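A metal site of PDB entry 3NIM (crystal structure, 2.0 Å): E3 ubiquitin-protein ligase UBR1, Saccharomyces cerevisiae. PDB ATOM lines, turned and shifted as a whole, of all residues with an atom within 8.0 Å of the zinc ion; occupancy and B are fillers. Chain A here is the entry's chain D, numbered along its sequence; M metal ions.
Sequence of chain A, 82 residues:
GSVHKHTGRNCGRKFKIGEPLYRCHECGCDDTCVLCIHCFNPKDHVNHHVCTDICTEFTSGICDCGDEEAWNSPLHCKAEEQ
The side-chain sulfur (SG) of Cys 24 lies close to a ring nitrogen (ND1) of His 48. A ring nitrogen (NE2) of His 48 sits at hydrogen-bond distance from the backbone carbonyl oxygen of Asp 44, at 3.2 Å. O of Cys 27 is in hydrogen-bond range of N of Asn 72, at 3.0 Å. The side-chain sulfur (SG) of Cys 24 sits close to the backbone NH (N) of Glu 26, 3.7 Å away.
O of Asp 44 touches the zinc ion, at 3.97 Å. Within 4 Å of the zinc ion: Cys 24, Cys 27, Asp 44, His 45 and His 48.
The zinc ion is bound by the side-chain sulfur (SG) of Cys 24 (2.0 Å), a ring nitrogen (ND1) of His 45 (2.1 Å) and the side-chain sulfur (SG) of Cys 27 (2.4 Å). Slightly farther from the zinc ion lies ND1 of His 48 (2.7 Å).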
ATOM      1  N   ARG A  23      -0.172  -1.241   0.927  1.00  0.00           N
ATOM      2  CA  ARG A  23       0.969  -1.038   1.825  1.00  0.00           C
ATOM      3  C   ARG A  23       0.474  -1.089   3.262  1.00  0.00           C
ATOM      4  O   ARG A  23      -0.617  -0.607   3.559  1.00  0.00           O
ATOM      5  CB  ARG A  23       1.635   0.317   1.569  1.00  0.00           C
ATOM      6  CG  ARG A  23       2.168   0.482   0.167  1.00  0.00           C
ATOM      7  CD  ARG A  23       3.182   1.612   0.061  1.00  0.00           C
ATOM      8  NE  ARG A  23       3.593   1.853  -1.322  1.00  0.00           N
ATOM      9  CZ  ARG A  23       2.811   2.441  -2.229  1.00  0.00           C
ATOM     10  NH1 ARG A  23       1.581   2.823  -1.915  1.00  0.00           N
ATOM     11  NH2 ARG A  23       3.256   2.621  -3.463  1.00  0.00           N
ATOM     12  N   CYS A  24       1.282  -1.673   4.142  1.00  0.00           N
ATOM     13  CA  CYS A  24       0.988  -1.712   5.561  1.00  0.00           C
ATOM     14  C   CYS A  24       2.198  -1.203   6.359  1.00  0.00           C
ATOM     15  O   CYS A  24       3.328  -1.627   6.097  1.00  0.00           O
ATOM     16  CB  CYS A  24       0.582  -3.134   5.977  1.00  0.00           C
ATOM     17  SG  CYS A  24       0.364  -3.409   7.756  1.00  0.00           S
ATOM     18  N   HIS A  25       1.966  -0.295   7.293  1.00  0.00           N
ATOM     19  CA  HIS A  25       3.051   0.286   8.088  1.00  0.00           C
ATOM     20  C   HIS A  25       3.679  -0.716   9.043  1.00  0.00           C
ATOM     21  O   HIS A  25       4.907  -0.775   9.173  1.00  0.00           O
ATOM     22  CB  HIS A  25       2.605   1.525   8.872  1.00  0.00           C
ATOM     23  CG  HIS A  25       3.723   2.227   9.573  1.00  0.00           C
ATOM     24  ND1 HIS A  25       4.171   1.851  10.824  1.00  0.00           N
ATOM     25  CD2 HIS A  25       4.509   3.265   9.191  1.00  0.00           C
ATOM     26  CE1 HIS A  25       5.178   2.629  11.186  1.00  0.00           C
ATOM     27  NE2 HIS A  25       5.401   3.494  10.210  1.00  0.00           N
ATOM     28  N   GLU A  26       2.850  -1.506   9.705  1.00  0.00           N
ATOM     29  CA  GLU A  26       3.327  -2.461  10.692  1.00  0.00           C
ATOM     30  C   GLU A  26       3.811  -3.772  10.063  1.00  0.00           C
ATOM     31  O   GLU A  26       4.057  -4.745  10.787  1.00  0.00           O
ATOM     32  CB  GLU A  26       2.250  -2.765  11.731  1.00  0.00           C
ATOM     33  CG  GLU A  26       1.796  -1.566  12.573  1.00  0.00           C
ATOM     34  CD  GLU A  26       0.828  -0.638  11.851  1.00  0.00           C
ATOM     35  OE1 GLU A  26       0.628   0.488  12.333  1.00  0.00           O
ATOM     36  OE2 GLU A  26       0.271  -1.036  10.808  1.00  0.00           O
ATOM     37  N   CYS A  27       3.949  -3.803   8.744  1.00  0.00           N
ATOM     38  CA  CYS A  27       4.378  -5.021   8.059  1.00  0.00           C
ATOM     39  C   CYS A  27       5.518  -4.792   7.072  1.00  0.00           C
ATOM     40  O   CYS A  27       6.514  -5.514   7.099  1.00  0.00           O
ATOM     41  CB  CYS A  27       3.192  -5.753   7.426  1.00  0.00           C
ATOM     42  SG  CYS A  27       2.107  -6.584   8.630  1.00  0.00           S
ATOM     43  N   GLY A  28       5.400  -3.777   6.215  1.00  0.00           N
ATOM     44  CA  GLY A  28       6.441  -3.437   5.252  1.00  0.00           C
ATOM     45  C   GLY A  28       7.675  -2.810   5.875  1.00  0.00           C
ATOM     46  O   GLY A  28       7.602  -1.704   6.442  1.00  0.00           O
ATOM     47  N   LEU A  35       1.567  -5.185  -1.651  1.00  0.00           N
ATOM     48  CA  LEU A  35       0.816  -6.414  -1.993  1.00  0.00           C
ATOM     49  C   LEU A  35      -0.229  -6.106  -3.033  1.00  0.00           C
ATOM     50  O   LEU A  35      -0.825  -5.025  -3.026  1.00  0.00           O
ATOM     51  CB  LEU A  35       0.144  -7.041  -0.756  1.00  0.00           C
ATOM     52  CG  LEU A  35       0.979  -7.517   0.440  1.00  0.00           C
ATOM     53  CD1 LEU A  35       0.143  -7.613   1.700  1.00  0.00           C
ATOM     54  CD2 LEU A  35       1.710  -8.836   0.190  1.00  0.00           C
ATOM     55  N   PHE A  40      -3.294  -9.506  -0.867  1.00  0.00           N
ATOM     56  CA  PHE A  40      -3.550  -8.805   0.391  1.00  0.00           C
ATOM     57  C   PHE A  40      -4.624  -9.525   1.226  1.00  0.00           C
ATOM     58  O   PHE A  40      -5.748  -9.731   0.774  1.00  0.00           O
ATOM     59  CB  PHE A  40      -3.955  -7.355   0.143  1.00  0.00           C
ATOM     60  CG  PHE A  40      -4.257  -6.598   1.396  1.00  0.00           C
ATOM     61  CD1 PHE A  40      -3.239  -6.091   2.176  1.00  0.00           C
ATOM     62  CD2 PHE A  40      -5.578  -6.392   1.785  1.00  0.00           C
ATOM     63  CE1 PHE A  40      -3.532  -5.360   3.341  1.00  0.00           C
ATOM     64  CE2 PHE A  40      -5.890  -5.688   2.943  1.00  0.00           C
ATOM     65  CZ  PHE A  40      -4.867  -5.192   3.729  1.00  0.00           C
ATOM     66  N   ASN A  41      -4.247  -9.920   2.438  1.00  0.00           N
ATOM     67  CA  ASN A  41      -5.146 -10.681   3.315  1.00  0.00           C
ATOM     68  C   ASN A  41      -5.610  -9.760   4.447  1.00  0.00           C
ATOM     69  O   ASN A  41      -4.808  -9.370   5.292  1.00  0.00           O
ATOM     70  CB  ASN A  41      -4.446 -11.946   3.846  1.00  0.00           C
ATOM     71  CG  ASN A  41      -5.418 -12.969   4.431  1.00  0.00           C
ATOM     72  OD1 ASN A  41      -6.627 -12.731   4.517  1.00  0.00           O
ATOM     73  ND2 ASN A  41      -4.887 -14.123   4.839  1.00  0.00           N
ATOM     74  N   PRO A  42      -6.895  -9.369   4.445  1.00  0.00           N
ATOM     75  CA  PRO A  42      -7.408  -8.460   5.476  1.00  0.00           C
ATOM     76  C   PRO A  42      -7.112  -8.911   6.909  1.00  0.00           C
ATOM     77  O   PRO A  42      -6.822  -8.063   7.759  1.00  0.00           O
ATOM     78  CB  PRO A  42      -8.919  -8.441   5.221  1.00  0.00           C
ATOM     79  CG  PRO A  42      -9.021  -8.715   3.773  1.00  0.00           C
ATOM     80  CD  PRO A  42      -7.943  -9.725   3.481  1.00  0.00           C
ATOM     81  N   LYS A  43      -7.149 -10.224   7.157  1.00  0.00           N
ATOM     82  CA  LYS A  43      -6.886 -10.795   8.493  1.00  0.00           C
ATOM     83  C   LYS A  43      -5.558 -10.387   9.067  1.00  0.00           C
ATOM     84  O   LYS A  43      -5.424 -10.186  10.273  1.00  0.00           O
ATOM     85  CB  LYS A  43      -6.908 -12.322   8.448  1.00  0.00           C
ATOM     86  CG  LYS A  43      -8.187 -12.971   8.022  1.00  0.00           C
ATOM     87  CD  LYS A  43      -7.974 -14.463   8.030  1.00  0.00           C
ATOM     88  CE  LYS A  43      -9.138 -15.201   7.419  1.00  0.00           C
ATOM     89  NZ  LYS A  43      -8.813 -16.648   7.277  1.00  0.00           N
ATOM     90  N   ASP A  44      -4.551 -10.283   8.187  1.00  0.00           N
ATOM     91  CA  ASP A  44      -3.191  -9.982   8.612  1.00  0.00           C
ATOM     92  C   ASP A  44      -3.058  -8.558   9.120  1.00  0.00           C
ATOM     93  O   ASP A  44      -2.163  -8.250   9.905  1.00  0.00           O
ATOM     94  CB  ASP A  44      -2.204 -10.232   7.452  1.00  0.00           C
ATOM     95  CG  ASP A  44      -2.157 -11.682   7.014  1.00  0.00           C
ATOM     96  OD1 ASP A  44      -2.349 -12.577   7.877  1.00  0.00           O
ATOM     97  OD2 ASP A  44      -1.918 -11.917   5.811  1.00  0.00           O
ATOM     98  N   HIS A  45      -3.977  -7.700   8.679  1.00  0.00           N
ATOM     99  CA  HIS A  45      -3.844  -6.271   8.925  1.00  0.00           C
ATOM    100  C   HIS A  45      -5.108  -5.665   9.578  1.00  0.00           C
ATOM    101  O   HIS A  45      -5.434  -4.498   9.358  1.00  0.00           O
ATOM    102  CB  HIS A  45      -3.456  -5.557   7.614  1.00  0.00           C
ATOM    103  CG  HIS A  45      -2.483  -6.337   6.776  1.00  0.00           C
ATOM    104  ND1 HIS A  45      -1.136  -6.356   7.032  1.00  0.00           N
ATOM    105  CD2 HIS A  45      -2.684  -7.154   5.718  1.00  0.00           C
ATOM    106  CE1 HIS A  45      -0.539  -7.135   6.147  1.00  0.00           C
ATOM    107  NE2 HIS A  45      -1.458  -7.630   5.339  1.00  0.00           N
ATOM    108  N   VAL A  46      -5.760  -6.478  10.412  1.00  0.00           N
ATOM    109  CA  VAL A  46      -6.985  -6.120  11.155  1.00  0.00           C
ATOM    110  C   VAL A  46      -6.869  -4.786  11.919  1.00  0.00           C
ATOM    111  O   VAL A  46      -7.718  -3.892  11.770  1.00  0.00           O
ATOM    112  CB  VAL A  46      -7.379  -7.260  12.150  1.00  0.00           C
ATOM    113  CG1 VAL A  46      -8.549  -6.829  13.030  1.00  0.00           C
ATOM    114  CG2 VAL A  46      -7.748  -8.522  11.408  1.00  0.00           C
ATOM    115  N   ASN A  47      -5.836  -4.643  12.727  1.00  0.00           N
ATOM    116  CA  ASN A  47      -5.606  -3.362  13.360  1.00  0.00           C
ATOM    117  C   ASN A  47      -4.216  -2.850  13.019  1.00  0.00           C
ATOM    118  O   ASN A  47      -3.390  -2.564  13.904  1.00  0.00           O
ATOM    119  CB  ASN A  47      -5.935  -3.374  14.870  1.00  0.00           C
ATOM    120  CG  ASN A  47      -5.377  -4.593  15.584  1.00  0.00           C
ATOM    121  OD1 ASN A  47      -4.156  -4.783  15.629  1.00  0.00           O
ATOM    122  ND2 ASN A  47      -6.266  -5.409  16.158  1.00  0.00           N
ATOM    123  N   HIS A  48      -3.976  -2.766  11.722  1.00  0.00           N
ATOM    124  CA  HIS A  48      -2.786  -2.169  11.134  1.00  0.00           C
ATOM    125  C   HIS A  48      -3.152  -0.930  10.329  1.00  0.00           C
ATOM    126  O   HIS A  48      -4.324  -0.688  10.031  1.00  0.00           O
ATOM    127  CB  HIS A  48      -2.102  -3.171  10.210  1.00  0.00           C
ATOM    128  CG  HIS A  48      -1.505  -4.353  10.922  1.00  0.00           C
ATOM    129  ND1 HIS A  48      -0.140  -4.575  10.984  1.00  0.00           N
ATOM    130  CD2 HIS A  48      -2.077  -5.380  11.597  1.00  0.00           C
ATOM    131  CE1 HIS A  48       0.091  -5.676  11.664  1.00  0.00           C
ATOM    132  NE2 HIS A  48      -1.064  -6.190  12.050  1.00  0.00           N
ATOM    133  N   HIS A  49      -2.139  -0.141   9.988  1.00  0.00           N
ATOM    134  CA  HIS A  49      -2.308   1.108   9.246  1.00  0.00           C
ATOM    135  C   HIS A  49      -2.030   0.867   7.765  1.00  0.00           C
ATOM    136  O   HIS A  49      -0.887   0.950   7.312  1.00  0.00           O
ATOM    137  CB  HIS A  49      -1.399   2.191   9.824  1.00  0.00           C
ATOM    138  CG  HIS A  49      -1.823   2.668  11.184  1.00  0.00           C
ATOM    139  ND1 HIS A  49      -1.653   1.901  12.319  1.00  0.00           N
ATOM    140  CD2 HIS A  49      -2.423   3.810  11.582  1.00  0.00           C
ATOM    141  CE1 HIS A  49      -2.124   2.564  13.362  1.00  0.00           C
ATOM    142  NE2 HIS A  49      -2.594   3.721  12.950  1.00  0.00           N
ATOM    143  N   VAL A  50      -3.085   0.556   7.017  1.00  0.00           N
ATOM    144  CA  VAL A  50      -2.970   0.142   5.619  1.00  0.00           C
ATOM    145  C   VAL A  50      -3.362   1.274   4.691  1.00  0.00           C
ATOM    146  O   VAL A  50      -4.342   1.983   4.934  1.00  0.00           O
ATOM    147  CB  VAL A  50      -3.853  -1.096   5.350  1.00  0.00           C
ATOM    148  CG1 VAL A  50      -3.838  -1.484   3.862  1.00  0.00           C
ATOM    149  CG2 VAL A  50      -3.391  -2.263   6.180  1.00  0.00           C
ATOM    150  N   TRP A  71       8.796  -8.497   4.699  1.00  0.00           N
ATOM    151  CA  TRP A  71       7.801  -8.336   5.757  1.00  0.00           C
ATOM    152  C   TRP A  71       8.335  -8.626   7.161  1.00  0.00           C
ATOM    153  O   TRP A  71       9.277  -9.414   7.321  1.00  0.00           O
ATOM    154  CB  TRP A  71       6.574  -9.198   5.446  1.00  0.00           C
ATOM    155  CG  TRP A  71       6.111  -9.015   4.031  1.00  0.00           C
ATOM    156  CD1 TRP A  71       6.316  -9.869   2.977  1.00  0.00           C
ATOM    157  CD2 TRP A  71       5.416  -7.881   3.486  1.00  0.00           C
ATOM    158  NE1 TRP A  71       5.767  -9.352   1.826  1.00  0.00           N
ATOM    159  CE2 TRP A  71       5.217  -8.123   2.117  1.00  0.00           C
ATOM    160  CE3 TRP A  71       4.938  -6.682   4.038  1.00  0.00           C
ATOM    161  CZ2 TRP A  71       4.556  -7.214   1.279  1.00  0.00           C
ATOM    162  CZ3 TRP A  71       4.286  -5.776   3.205  1.00  0.00           C
ATOM    163  CH2 TRP A  71       4.103  -6.058   1.846  1.00  0.00           C
ATOM    164  N   ASN A  72       7.723  -7.995   8.158  1.00  0.00           N
ATOM    165  CA  ASN A  72       8.088  -8.132   9.567  1.00  0.00           C
ATOM    166  C   ASN A  72       7.438  -9.330  10.274  1.00  0.00           C
ATOM    167  O   ASN A  72       7.765  -9.611  11.435  1.00  0.00           O
ATOM    168  CB  ASN A  72       7.745  -6.856  10.337  1.00  0.00           C
ATOM    169  CG  ASN A  72       8.423  -5.621   9.748  1.00  0.00           C
ATOM    170  OD1 ASN A  72       9.547  -5.696   9.263  1.00  0.00           O
ATOM    171  ND2 ASN A  72       7.741  -4.486   9.806  1.00  0.00           N
ATOM    172  N   SER A  73       6.531 -10.019   9.582  1.00  0.00           N
ATOM    173  CA  SER A  73       5.836 -11.186  10.137  1.00  0.00           C
ATOM    174  C   SER A  73       5.217 -12.026   9.027  1.00  0.00           C
ATOM    175  O   SER A  73       5.025 -11.537   7.918  1.00  0.00           O
ATOM    176  CB  SER A  73       4.768 -10.749  11.150  1.00  0.00           C
ATOM    177  OG  SER A  73       3.932  -9.727  10.615  1.00  0.00           O
ATOM    178  N   LEU A  75       2.909 -13.523   6.520  1.00  0.00           N
ATOM    179  CA  LEU A  75       1.650 -13.194   5.886  1.00  0.00           C
ATOM    180  C   LEU A  75       0.977 -14.474   5.444  1.00  0.00           C
ATOM    181  O   LEU A  75       1.602 -15.541   5.362  1.00  0.00           O
ATOM    182  CB  LEU A  75       1.874 -12.256   4.701  1.00  0.00           C
ATOM    183  CG  LEU A  75       2.709 -10.981   4.883  1.00  0.00           C
ATOM    184  CD1 LEU A  75       3.005 -10.379   3.530  1.00  0.00           C
ATOM    185  CD2 LEU A  75       2.048  -9.938   5.787  1.00  0.00           C
HETATM  186 ZN    ZN M   1       0.031  -5.320   8.371  1.00  0.00          ZN
